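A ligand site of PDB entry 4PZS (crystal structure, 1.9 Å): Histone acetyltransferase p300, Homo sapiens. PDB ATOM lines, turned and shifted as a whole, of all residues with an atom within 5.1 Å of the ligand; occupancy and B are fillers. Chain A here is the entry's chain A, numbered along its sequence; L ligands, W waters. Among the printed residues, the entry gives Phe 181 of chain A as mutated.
O17 of the ligand sits close to O of Trp 150.
N of Pro 172 sits close to N4 of the ligand (3.4 Å).
Residues that only touch the ligand: Ile 109 (3.1 Å), Tyr 128 (3.3 Å), Pro 154 (3.4 Å), Cys 152 (3.5 Å), Tyr 111 (3.5 Å), Lys 170 (3.5 Å), Tyr 160 (3.6 Å), Asp 113 (3.7 Å), Leu 177 (3.8 Å) and Pro 153 (3.9 Å).
Hydrophobic or aromatic side chains that line the ligand: Ile 109, Leu 112, Tyr 128, Pro 154, Tyr 160, Pro 172, Leu 177 and Trp 180.
19 residues have an atom within 4 Å of the ligand: Ile 109, Tyr 111, Leu 112, Asp 113, Ser 114, Arg 124, Thr 125, Tyr 128, Trp 150, Cys 152, Pro 153, Pro 154, Tyr 160, Lys 170, Ile 171, Pro 172, Arg 176, Leu 177 and Trp 180.
The side-chain hydroxyl of Tyr 128 sits close to the side-chain hydroxyl of Ser 114 (3.3 Å).
The side-chain amide nitrogen (NE2) of Gln 169 sits at hydrogen-bond distance from the backbone carbonyl oxygen (O) of Ser 114, 3.0 Å away.
The side-chain hydroxyl of Tyr 160 lies within hydrogen-bond range of the backbone carbonyl oxygen of Cys 152.
OH of Tyr 160 lies close to O of Pro 153 (3.4 Å).
Water W6 lies within hydrogen-bond range of an oxygen (O1) of the ligand (2.7 Å) and the backbone NH of Lys 170 (2.8 Å).
Water W8 lies within hydrogen-bond range of the backbone carbonyl oxygen of Lys 170 and an oxygen (O8) of the ligand.
Water W3 lies within hydrogen-bond range of O of Lys 170 (2.8 Å), O14 of the ligand (2.9 Å) and NE2 of Gln 169 (3.1 Å).
Water W4 bridges O9 of the ligand (2.9 Å) and NH1 of Arg 176 (3.2 Å).
Water W5 bridges NH1 of Arg 124 (2.9 Å) and O5 of the ligand (3.0 Å).
An oxygen (O12) of the ligand is in hydrogen-bond range of the side-chain hydroxyl (OG1) of Thr 125, 2.6 Å away.
O15 of the ligand sits at hydrogen-bond distance from N of Ser 114 (3.1 Å).
O15 of the ligand is in hydrogen-bond range of OG of Ser 114 (2.8 Å).
The guanidinium group (NE) of Arg 124 lies within salt-bridge range of an oxygen (O11) of the ligand (2.8 Å).
The backbone carbonyl oxygen (O) of Ile 171 sits at hydrogen-bond distance from a nitrogen (N3) of the ligand, at 2.9 Å.
The indole nitrogen (NE1) of Trp 180 is in hydrogen-bond range of an oxygen (O12) of the ligand.
An oxygen (O6) of the ligand sits at hydrogen-bond distance from the guanidinium group (NH1) of Arg 176, at 3.0 Å.
N of Leu 112 sits close to S1 of the ligand, at 3.7 Å.
N7 of the ligand sits at hydrogen-bond distance from O of Leu 112 (3.1 Å).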
ATOM      1  N   ILE A 109     -11.510  25.612 -17.651  1.00  0.00           N
ATOM      2  CA  ILE A 109     -12.651  24.981 -17.029  1.00  0.00           C
ATOM      3  C   ILE A 109     -12.785  25.529 -15.615  1.00  0.00           C
ATOM      4  O   ILE A 109     -11.901  25.341 -14.775  1.00  0.00           O
ATOM      5  CB  ILE A 109     -12.533  23.431 -16.998  1.00  0.00           C
ATOM      6  CG1 ILE A 109     -12.203  22.902 -18.397  1.00  0.00           C
ATOM      7  CG2 ILE A 109     -13.837  22.826 -16.489  1.00  0.00           C
ATOM      8  CD1 ILE A 109     -12.201  21.359 -18.498  1.00  0.00           C
ATOM      9  N   SER A 110     -13.890  26.219 -15.341  1.00  0.00           N
ATOM     10  CA  SER A 110     -14.139  26.716 -13.996  1.00  0.00           C
ATOM     11  C   SER A 110     -14.331  25.521 -13.055  1.00  0.00           C
ATOM     12  O   SER A 110     -13.650  25.378 -12.047  1.00  0.00           O
ATOM     13  CB  SER A 110     -15.366  27.629 -13.959  1.00  0.00           C
ATOM     14  OG  SER A 110     -15.225  28.726 -14.838  1.00  0.00           O
ATOM     15  N   TYR A 111     -15.275  24.663 -13.408  1.00  0.00           N
ATOM     16  CA  TYR A 111     -15.555  23.485 -12.614  1.00  0.00           C
ATOM     17  C   TYR A 111     -16.424  22.515 -13.385  1.00  0.00           C
ATOM     18  O   TYR A 111     -17.097  22.880 -14.360  1.00  0.00           O
ATOM     19  CB  TYR A 111     -16.234  23.852 -11.279  1.00  0.00           C
ATOM     20  CG  TYR A 111     -16.962  25.175 -11.253  1.00  0.00           C
ATOM     21  CD1 TYR A 111     -18.195  25.330 -11.886  1.00  0.00           C
ATOM     22  CD2 TYR A 111     -16.428  26.282 -10.597  1.00  0.00           C
ATOM     23  CE1 TYR A 111     -18.863  26.552 -11.858  1.00  0.00           C
ATOM     24  CE2 TYR A 111     -17.095  27.505 -10.559  1.00  0.00           C
ATOM     25  CZ  TYR A 111     -18.318  27.629 -11.193  1.00  0.00           C
ATOM     26  OH  TYR A 111     -18.977  28.841 -11.176  1.00  0.00           O
ATOM     27  N   LEU A 112     -16.374  21.256 -12.953  1.00  0.00           N
ATOM     28  CA  LEU A 112     -17.234  20.222 -13.511  1.00  0.00           C
ATOM     29  C   LEU A 112     -17.653  19.313 -12.372  1.00  0.00           C
ATOM     30  O   LEU A 112     -16.996  19.240 -11.331  1.00  0.00           O
ATOM     31  CB  LEU A 112     -16.517  19.440 -14.617  1.00  0.00           C
ATOM     32  CG  LEU A 112     -15.379  18.458 -14.250  1.00  0.00           C
ATOM     33  CD1 LEU A 112     -15.891  17.113 -13.723  1.00  0.00           C
ATOM     34  CD2 LEU A 112     -14.485  18.233 -15.475  1.00  0.00           C
ATOM     35  N   ASP A 113     -18.762  18.609 -12.578  1.00  0.00           N
ATOM     36  CA  ASP A 113     -19.324  17.819 -11.508  1.00  0.00           C
ATOM     37  C   ASP A 113     -20.151  16.722 -12.151  1.00  0.00           C
ATOM     38  O   ASP A 113     -20.574  16.852 -13.308  1.00  0.00           O
ATOM     39  CB  ASP A 113     -20.168  18.705 -10.595  1.00  0.00           C
ATOM     40  CG  ASP A 113     -20.519  18.052  -9.262  1.00  0.00           C
ATOM     41  OD1 ASP A 113     -19.893  17.051  -8.862  1.00  0.00           O
ATOM     42  OD2 ASP A 113     -21.410  18.602  -8.595  1.00  0.00           O
ATOM     43  N   SER A 114     -20.370  15.642 -11.421  1.00  0.00           N
ATOM     44  CA  SER A 114     -21.209  14.560 -11.910  1.00  0.00           C
ATOM     45  C   SER A 114     -21.909  13.862 -10.767  1.00  0.00           C
ATOM     46  O   SER A 114     -21.493  13.943  -9.604  1.00  0.00           O
ATOM     47  CB  SER A 114     -20.367  13.538 -12.667  1.00  0.00           C
ATOM     48  OG  SER A 114     -19.477  12.880 -11.775  1.00  0.00           O
ATOM     49  N   LYS A 121     -22.849   1.446 -16.017  1.00  0.00           N
ATOM     50  CA  LYS A 121     -21.691   1.817 -15.202  1.00  0.00           C
ATOM     51  C   LYS A 121     -20.378   1.774 -15.969  1.00  0.00           C
ATOM     52  O   LYS A 121     -19.568   2.686 -15.857  1.00  0.00           O
ATOM     53  CB  LYS A 121     -21.585   0.879 -13.976  1.00  0.00           C
ATOM     54  CG  LYS A 121     -22.550   1.181 -12.872  1.00  0.00           C
ATOM     55  CD  LYS A 121     -22.468   0.130 -11.770  1.00  0.00           C
ATOM     56  CE  LYS A 121     -21.049  -0.017 -11.233  1.00  0.00           C
ATOM     57  NZ  LYS A 121     -21.093  -0.408  -9.790  1.00  0.00           N
ATOM     58  N   ARG A 124     -19.469   4.948 -18.011  1.00  0.00           N
ATOM     59  CA  ARG A 124     -19.591   6.285 -17.394  1.00  0.00           C
ATOM     60  C   ARG A 124     -18.330   7.148 -17.586  1.00  0.00           C
ATOM     61  O   ARG A 124     -18.416   8.275 -18.099  1.00  0.00           O
ATOM     62  CB  ARG A 124     -19.907   6.147 -15.888  1.00  0.00           C
ATOM     63  CG  ARG A 124     -20.059   7.487 -15.154  1.00  0.00           C
ATOM     64  CD  ARG A 124     -20.157   7.289 -13.626  1.00  0.00           C
ATOM     65  NE  ARG A 124     -18.876   6.882 -13.056  1.00  0.00           N
ATOM     66  CZ  ARG A 124     -18.550   5.630 -12.726  1.00  0.00           C
ATOM     67  NH1 ARG A 124     -19.411   4.646 -12.898  1.00  0.00           N
ATOM     68  NH2 ARG A 124     -17.359   5.382 -12.205  1.00  0.00           N
ATOM     69  N   THR A 125     -17.170   6.637 -17.174  1.00  0.00           N
ATOM     70  CA  THR A 125     -15.930   7.403 -17.259  1.00  0.00           C
ATOM     71  C   THR A 125     -15.605   7.703 -18.720  1.00  0.00           C
ATOM     72  O   THR A 125     -15.202   8.814 -19.057  1.00  0.00           O
ATOM     73  CB  THR A 125     -14.716   6.659 -16.596  1.00  0.00           C
ATOM     74  OG1 THR A 125     -14.926   6.558 -15.182  1.00  0.00           O
ATOM     75  CG2 THR A 125     -13.416   7.430 -16.855  1.00  0.00           C
ATOM     76  N   TYR A 128     -17.717  10.638 -19.816  1.00  0.00           N
ATOM     77  CA  TYR A 128     -17.138  11.891 -19.304  1.00  0.00           C
ATOM     78  C   TYR A 128     -15.985  12.346 -20.188  1.00  0.00           C
ATOM     79  O   TYR A 128     -15.906  13.515 -20.580  1.00  0.00           O
ATOM     80  CB  TYR A 128     -16.639  11.770 -17.847  1.00  0.00           C
ATOM     81  CG  TYR A 128     -17.700  11.470 -16.801  1.00  0.00           C
ATOM     82  CD1 TYR A 128     -19.034  11.847 -16.994  1.00  0.00           C
ATOM     83  CD2 TYR A 128     -17.367  10.821 -15.624  1.00  0.00           C
ATOM     84  CE1 TYR A 128     -19.998  11.565 -16.027  1.00  0.00           C
ATOM     85  CE2 TYR A 128     -18.339  10.539 -14.645  1.00  0.00           C
ATOM     86  CZ  TYR A 128     -19.638  10.916 -14.865  1.00  0.00           C
ATOM     87  OH  TYR A 128     -20.593  10.643 -13.911  1.00  0.00           O
ATOM     88  N   ILE A 149      -6.635  23.481 -16.989  1.00  0.00           N
ATOM     89  CA  ILE A 149      -7.386  22.699 -16.008  1.00  0.00           C
ATOM     90  C   ILE A 149      -6.711  22.685 -14.646  1.00  0.00           C
ATOM     91  O   ILE A 149      -5.511  22.426 -14.523  1.00  0.00           O
ATOM     92  CB  ILE A 149      -7.586  21.255 -16.492  1.00  0.00           C
ATOM     93  CG1 ILE A 149      -8.553  21.225 -17.667  1.00  0.00           C
ATOM     94  CG2 ILE A 149      -8.077  20.377 -15.361  1.00  0.00           C
ATOM     95  CD1 ILE A 149      -8.520  19.934 -18.441  1.00  0.00           C
ATOM     96  N   TRP A 150      -7.497  22.994 -13.616  1.00  0.00           N
ATOM     97  CA  TRP A 150      -7.089  22.891 -12.213  1.00  0.00           C
ATOM     98  C   TRP A 150      -7.698  21.597 -11.660  1.00  0.00           C
ATOM     99  O   TRP A 150      -8.913  21.524 -11.467  1.00  0.00           O
ATOM    100  CB  TRP A 150      -7.582  24.133 -11.454  1.00  0.00           C
ATOM    101  CG  TRP A 150      -7.290  24.193  -9.964  1.00  0.00           C
ATOM    102  CD1 TRP A 150      -6.512  23.341  -9.239  1.00  0.00           C
ATOM    103  CD2 TRP A 150      -7.786  25.169  -9.045  1.00  0.00           C
ATOM    104  NE1 TRP A 150      -6.502  23.717  -7.919  1.00  0.00           N
ATOM    105  CE2 TRP A 150      -7.271  24.853  -7.768  1.00  0.00           C
ATOM    106  CE3 TRP A 150      -8.614  26.298  -9.168  1.00  0.00           C
ATOM    107  CZ2 TRP A 150      -7.555  25.605  -6.628  1.00  0.00           C
ATOM    108  CZ3 TRP A 150      -8.901  27.049  -8.038  1.00  0.00           C
ATOM    109  CH2 TRP A 150      -8.371  26.702  -6.793  1.00  0.00           C
ATOM    110  N   ALA A 151      -6.885  20.571 -11.456  1.00  0.00           N
ATOM    111  CA  ALA A 151      -7.423  19.273 -11.017  1.00  0.00           C
ATOM    112  C   ALA A 151      -7.687  19.274  -9.515  1.00  0.00           C
ATOM    113  O   ALA A 151      -7.013  18.604  -8.746  1.00  0.00           O
ATOM    114  CB  ALA A 151      -6.449  18.131 -11.378  1.00  0.00           C
ATOM    115  N   CYS A 152      -8.686  20.047  -9.109  1.00  0.00           N
ATOM    116  CA  CYS A 152      -8.972  20.217  -7.678  1.00  0.00           C
ATOM    117  C   CYS A 152     -10.236  19.491  -7.224  1.00  0.00           C
ATOM    118  O   CYS A 152     -11.331  19.925  -7.504  1.00  0.00           O
ATOM    119  CB  CYS A 152      -9.135  21.696  -7.343  1.00  0.00           C
ATOM    120  SG  CYS A 152      -9.298  21.965  -5.571  1.00  0.00           S
ATOM    121  N   PRO A 153     -10.071  18.370  -6.503  1.00  0.00           N
ATOM    122  CA  PRO A 153     -11.269  17.716  -5.971  1.00  0.00           C
ATOM    123  C   PRO A 153     -11.930  18.567  -4.887  1.00  0.00           C
ATOM    124  O   PRO A 153     -11.233  19.295  -4.159  1.00  0.00           O
ATOM    125  CB  PRO A 153     -10.735  16.410  -5.393  1.00  0.00           C
ATOM    126  CG  PRO A 153      -9.308  16.676  -5.102  1.00  0.00           C
ATOM    127  CD  PRO A 153      -8.825  17.688  -6.112  1.00  0.00           C
ATOM    128  N   PRO A 154     -13.270  18.482  -4.762  1.00  0.00           N
ATOM    129  CA  PRO A 154     -14.019  19.251  -3.771  1.00  0.00           C
ATOM    130  C   PRO A 154     -13.745  18.768  -2.364  1.00  0.00           C
ATOM    131  O   PRO A 154     -13.473  17.593  -2.168  1.00  0.00           O
ATOM    132  CB  PRO A 154     -15.486  19.012  -4.167  1.00  0.00           C
ATOM    133  CG  PRO A 154     -15.471  17.712  -4.878  1.00  0.00           C
ATOM    134  CD  PRO A 154     -14.129  17.572  -5.536  1.00  0.00           C
ATOM    135  N   TYR A 160     -19.821  20.858  -6.099  1.00  0.00           N
ATOM    136  CA  TYR A 160     -19.464  21.881  -7.077  1.00  0.00           C
ATOM    137  C   TYR A 160     -20.705  22.424  -7.769  1.00  0.00           C
ATOM    138  O   TYR A 160     -20.943  23.635  -7.779  1.00  0.00           O
ATOM    139  CB  TYR A 160     -18.467  21.341  -8.109  1.00  0.00           C
ATOM    140  CG  TYR A 160     -17.044  21.312  -7.605  1.00  0.00           C
ATOM    141  CD1 TYR A 160     -16.706  21.915  -6.392  1.00  0.00           C
ATOM    142  CD2 TYR A 160     -16.020  20.701  -8.325  1.00  0.00           C
ATOM    143  CE1 TYR A 160     -15.412  21.905  -5.926  1.00  0.00           C
ATOM    144  CE2 TYR A 160     -14.726  20.681  -7.860  1.00  0.00           C
ATOM    145  CZ  TYR A 160     -14.421  21.294  -6.661  1.00  0.00           C
ATOM    146  OH  TYR A 160     -13.123  21.275  -6.175  1.00  0.00           O
ATOM    147  N   GLN A 169     -21.059   7.886  -3.501  1.00  0.00           N
ATOM    148  CA  GLN A 169     -20.210   8.364  -4.604  1.00  0.00           C
ATOM    149  C   GLN A 169     -18.905   8.908  -4.044  1.00  0.00           C
ATOM    150  O   GLN A 169     -18.858  10.003  -3.492  1.00  0.00           O
ATOM    151  CB  GLN A 169     -20.915   9.443  -5.440  1.00  0.00           C
ATOM    152  CG  GLN A 169     -20.024   9.961  -6.593  1.00  0.00           C
ATOM    153  CD  GLN A 169     -20.752  10.886  -7.553  1.00  0.00           C
ATOM    154  OE1 GLN A 169     -21.951  10.752  -7.767  1.00  0.00           O
ATOM    155  NE2 GLN A 169     -20.020  11.829  -8.139  1.00  0.00           N
ATOM    156  N   LYS A 170     -17.827   8.122  -4.179  1.00  0.00           N
ATOM    157  CA  LYS A 170     -16.525   8.515  -3.635  1.00  0.00           C
ATOM    158  C   LYS A 170     -15.941   9.755  -4.324  1.00  0.00           C
ATOM    159  O   LYS A 170     -16.141   9.953  -5.533  1.00  0.00           O
ATOM    160  CB  LYS A 170     -15.525   7.370  -3.736  1.00  0.00           C
ATOM    161  CG  LYS A 170     -15.950   6.080  -3.013  1.00  0.00           C
ATOM    162  CD  LYS A 170     -14.770   5.110  -2.918  1.00  0.00           C
ATOM    163  CE  LYS A 170     -15.126   3.831  -2.148  1.00  0.00           C
ATOM    164  NZ  LYS A 170     -16.139   3.012  -2.876  1.00  0.00           N
ATOM    165  N   ILE A 171     -15.237  10.575  -3.559  1.00  0.00           N
ATOM    166  CA  ILE A 171     -14.509  11.709  -4.119  1.00  0.00           C
ATOM    167  C   ILE A 171     -13.050  11.320  -4.355  1.00  0.00           C
ATOM    168  O   ILE A 171     -12.367  10.854  -3.440  1.00  0.00           O
ATOM    169  CB  ILE A 171     -14.564  12.945  -3.187  1.00  0.00           C
ATOM    170  CG1 ILE A 171     -16.007  13.230  -2.748  1.00  0.00           C
ATOM    171  CG2 ILE A 171     -13.941  14.156  -3.882  1.00  0.00           C
ATOM    172  CD1 ILE A 171     -16.956  13.550  -3.894  1.00  0.00           C
ATOM    173  N   PRO A 172     -12.574  11.496  -5.596  1.00  0.00           N
ATOM    174  CA  PRO A 172     -11.195  11.096  -5.878  1.00  0.00           C
ATOM    175  C   PRO A 172     -10.196  11.935  -5.117  1.00  0.00           C
ATOM    176  O   PRO A 172     -10.428  13.113  -4.872  1.00  0.00           O
ATOM    177  CB  PRO A 172     -11.063  11.334  -7.393  1.00  0.00           C
ATOM    178  CG  PRO A 172     -12.096  12.379  -7.690  1.00  0.00           C
ATOM    179  CD  PRO A 172     -13.242  12.075  -6.771  1.00  0.00           C
ATOM    180  N   LYS A 173      -9.091  11.334  -4.723  1.00  0.00           N
ATOM    181  CA  LYS A 173      -8.006  12.098  -4.149  1.00  0.00           C
ATOM    182  C   LYS A 173      -7.326  12.816  -5.299  1.00  0.00           C
ATOM    183  O   LYS A 173      -7.562  12.484  -6.467  1.00  0.00           O
ATOM    184  CB  LYS A 173      -7.029  11.196  -3.388  1.00  0.00           C
ATOM    185  CG  LYS A 173      -7.525  10.734  -2.024  1.00  0.00           C
ATOM    186  CD  LYS A 173      -7.325  11.823  -0.971  1.00  0.00           C
ATOM    187  CE  LYS A 173      -7.683  11.341   0.429  1.00  0.00           C
ATOM    188  NZ  LYS A 173      -9.127  10.987   0.550  1.00  0.00           N
ATOM    189  N   ARG A 176      -5.547  10.580  -7.944  1.00  0.00           N
ATOM    190  CA  ARG A 176      -6.518   9.889  -8.785  1.00  0.00           C
ATOM    191  C   ARG A 176      -7.161  10.812  -9.831  1.00  0.00           C
ATOM    192  O   ARG A 176      -7.297  10.440 -11.007  1.00  0.00           O
ATOM    193  CB  ARG A 176      -7.626   9.254  -7.925  1.00  0.00           C
ATOM    194  CG  ARG A 176      -8.739   8.622  -8.762  1.00  0.00           C
ATOM    195  CD  ARG A 176      -9.782   7.958  -7.883  1.00  0.00           C
ATOM    196  NE  ARG A 176      -9.246   6.795  -7.187  1.00  0.00           N
ATOM    197  CZ  ARG A 176      -9.215   5.571  -7.698  1.00  0.00           C
ATOM    198  NH1 ARG A 176      -9.703   5.349  -8.915  1.00  0.00           N
ATOM    199  NH2 ARG A 176      -8.708   4.569  -7.001  1.00  0.00           N
ATOM    200  N   LEU A 177      -7.551  12.015  -9.396  1.00  0.00           N
ATOM    201  CA  LEU A 177      -8.135  13.012 -10.292  1.00  0.00           C
ATOM    202  C   LEU A 177      -7.111  13.482 -11.326  1.00  0.00           C
ATOM    203  O   LEU A 177      -7.435  13.681 -12.492  1.00  0.00           O
ATOM    204  CB  LEU A 177      -8.663  14.204  -9.495  1.00  0.00           C
ATOM    205  CG  LEU A 177      -9.364  15.304 -10.312  1.00  0.00           C
ATOM    206  CD1 LEU A 177     -10.594  14.727 -11.017  1.00  0.00           C
ATOM    207  CD2 LEU A 177      -9.780  16.470  -9.403  1.00  0.00           C
ATOM    208  N   TRP A 180      -6.834  10.831 -13.888  1.00  0.00           N
ATOM    209  CA  TRP A 180      -8.089  10.853 -14.636  1.00  0.00           C
ATOM    210  C   TRP A 180      -8.009  11.841 -15.795  1.00  0.00           C
ATOM    211  O   TRP A 180      -8.271  11.461 -16.937  1.00  0.00           O
ATOM    212  CB  TRP A 180      -9.226  11.190 -13.695  1.00  0.00           C
ATOM    213  CG  TRP A 180     -10.650  11.097 -14.255  1.00  0.00           C
ATOM    214  CD1 TRP A 180     -11.476   9.999 -14.228  1.00  0.00           C
ATOM    215  CD2 TRP A 180     -11.428  12.164 -14.823  1.00  0.00           C
ATOM    216  NE1 TRP A 180     -12.700  10.317 -14.765  1.00  0.00           N
ATOM    217  CE2 TRP A 180     -12.708  11.637 -15.134  1.00  0.00           C
ATOM    218  CE3 TRP A 180     -11.165  13.526 -15.101  1.00  0.00           C
ATOM    219  CZ2 TRP A 180     -13.716  12.413 -15.724  1.00  0.00           C
ATOM    220  CZ3 TRP A 180     -12.170  14.292 -15.680  1.00  0.00           C
ATOM    221  CH2 TRP A 180     -13.437  13.736 -15.973  1.00  0.00           C
ATOM    222  N   PHE A 181      -7.624  13.089 -15.513  1.00  0.00           N
ATOM    223  CA  PHE A 181      -7.372  14.080 -16.562  1.00  0.00           C
ATOM    224  C   PHE A 181      -6.256  13.653 -17.507  1.00  0.00           C
ATOM    225  O   PHE A 181      -6.353  13.890 -18.716  1.00  0.00           O
ATOM    226  CB  PHE A 181      -7.049  15.467 -15.956  1.00  0.00           C
ATOM    227  CG  PHE A 181      -8.247  16.222 -15.473  1.00  0.00           C
ATOM    228  CD1 PHE A 181      -9.192  16.689 -16.381  1.00  0.00           C
ATOM    229  CD2 PHE A 181      -8.455  16.439 -14.119  1.00  0.00           C
ATOM    230  CE1 PHE A 181     -10.317  17.373 -15.939  1.00  0.00           C
ATOM    231  CE2 PHE A 181      -9.576  17.124 -13.658  1.00  0.00           C
ATOM    232  CZ  PHE A 181     -10.514  17.601 -14.577  1.00  0.00           C
HETATM  233  N1  LIG L   1     -10.939   5.931  -3.010  1.00  0.00           N
HETATM  234  C1  LIG L   1     -11.134   4.754  -3.644  1.00  0.00           C
HETATM  235  N2  LIG L   1     -11.777   4.713  -4.827  1.00  0.00           N
HETATM  236  C2  LIG L   1     -12.241   5.858  -5.404  1.00  0.00           C
HETATM  237  C3  LIG L   1     -12.049   7.085  -4.791  1.00  0.00           C
HETATM  238  C4  LIG L   1     -11.384   7.088  -3.539  1.00  0.00           C
HETATM  239  N3  LIG L   1     -11.158   8.337  -2.851  1.00  0.00           N
HETATM  240  N4  LIG L   1     -12.607   8.055  -5.599  1.00  0.00           N
HETATM  241  C5  LIG L   1     -13.124   7.446  -6.678  1.00  0.00           C
HETATM  242  N5  LIG L   1     -12.899   6.128  -6.572  1.00  0.00           N
HETATM  243  C6  LIG L   1     -13.296   5.102  -7.540  1.00  0.00           C
HETATM  244  C7  LIG L   1     -14.752   5.155  -7.885  1.00  0.00           C
HETATM  245  O1  LIG L   1     -15.476   4.543  -6.872  1.00  0.00           O
HETATM  246  C8  LIG L   1     -14.840   4.481  -9.122  1.00  0.00           C
HETATM  247  O2  LIG L   1     -14.882   3.096  -8.915  1.00  0.00           O
HETATM  248  P1  LIG L   1     -15.532   2.168  -9.991  1.00  0.00           P
HETATM  249  O3  LIG L   1     -15.161   0.744  -9.746  1.00  0.00           O
HETATM  250  O4  LIG L   1     -15.052   2.540 -11.381  1.00  0.00           O
HETATM  251  O5  LIG L   1     -17.028   2.343  -9.895  1.00  0.00           O
HETATM  252  C9  LIG L   1     -13.580   4.811  -9.809  1.00  0.00           C
HETATM  253  O6  LIG L   1     -12.663   5.157  -8.806  1.00  0.00           O
HETATM  254  C10 LIG L   1     -13.736   5.999 -10.646  1.00  0.00           C
HETATM  255  O7  LIG L   1     -14.135   7.139  -9.923  1.00  0.00           O
HETATM  256  P2  LIG L   1     -13.751   8.627 -10.378  1.00  0.00           P
HETATM  257  O8  LIG L   1     -14.554   9.602  -9.526  1.00  0.00           O
HETATM  258  O9  LIG L   1     -12.266   8.859 -10.219  1.00  0.00           O
HETATM  259  O10 LIG L   1     -14.036   8.765 -11.947  1.00  0.00           O
HETATM  260  P3  LIG L   1     -15.395   9.068 -12.663  1.00  0.00           P
HETATM  261  O11 LIG L   1     -16.510   8.151 -12.221  1.00  0.00           O
HETATM  262  O12 LIG L   1     -15.149   8.937 -14.148  1.00  0.00           O
HETATM  263  O13 LIG L   1     -15.829  10.539 -12.308  1.00  0.00           O
HETATM  264  C11 LIG L   1     -15.455  12.941 -11.851  1.00  0.00           C
HETATM  265  C12 LIG L   1     -14.896  11.615 -12.415  1.00  0.00           C
HETATM  266  C13 LIG L   1     -16.430  13.496 -12.867  1.00  0.00           C
HETATM  267  C14 LIG L   1     -14.313  13.985 -11.650  1.00  0.00           C
HETATM  268  C15 LIG L   1     -16.131  12.660 -10.479  1.00  0.00           C
HETATM  269  O14 LIG L   1     -15.231  12.062  -9.590  1.00  0.00           O
HETATM  270  C16 LIG L   1     -16.703  13.928  -9.869  1.00  0.00           C
HETATM  271  O15 LIG L   1     -17.737  14.399 -10.262  1.00  0.00           O
HETATM  272  N6  LIG L   1     -15.998  14.565  -8.815  1.00  0.00           N
HETATM  273  C17 LIG L   1     -16.496  15.805  -8.137  1.00  0.00           C
HETATM  274  C18 LIG L   1     -16.061  17.088  -8.750  1.00  0.00           C
HETATM  275  C19 LIG L   1     -14.650  17.112  -9.262  1.00  0.00           C
HETATM  276  O16 LIG L   1     -13.785  16.436  -8.680  1.00  0.00           O
HETATM  277  N7  LIG L   1     -14.350  17.880 -10.436  1.00  0.00           N
HETATM  278  C20 LIG L   1     -13.033  17.933 -10.963  1.00  0.00           C
HETATM  279  C21 LIG L   1     -12.299  19.238 -10.776  1.00  0.00           C
HETATM  280  S1  LIG L   1     -13.111  20.703 -11.379  1.00  0.00           S
HETATM  281  C22 LIG L   1     -12.532  20.967 -13.058  1.00  0.00           C
HETATM  282  O17 LIG L   1     -11.529  21.690 -13.271  1.00  0.00           O
HETATM  283  C23 LIG L   1     -13.468  20.807 -14.225  1.00  0.00           C
HETATM  284  O   HOH W   1     -11.107  11.130 -10.858  1.00  0.00           O
HETATM  285  O   HOH W   2      -8.333   8.256  -4.911  1.00  0.00           O
HETATM  286  O   HOH W   3     -17.053  11.855  -7.370  1.00  0.00           O
HETATM  287  O   HOH W   4     -10.199   7.212 -11.417  1.00  0.00           O
HETATM  288  O   HOH W   5     -18.427   1.935 -12.476  1.00  0.00           O
HETATM  289  O   HOH W   6     -17.613   5.885  -5.877  1.00  0.00           O
HETATM  290  O   HOH W   7     -18.069   8.626  -9.925  1.00  0.00           O
HETATM  291  O   HOH W   8     -16.272   8.352  -7.754  1.00  0.00           O
HETATM  292  O   HOH W   9     -14.899  -1.072 -11.749  1.00  0.00           O
HETATM  293  O   HOH W  10      -7.968   6.372  -2.792  1.00  0.00           O
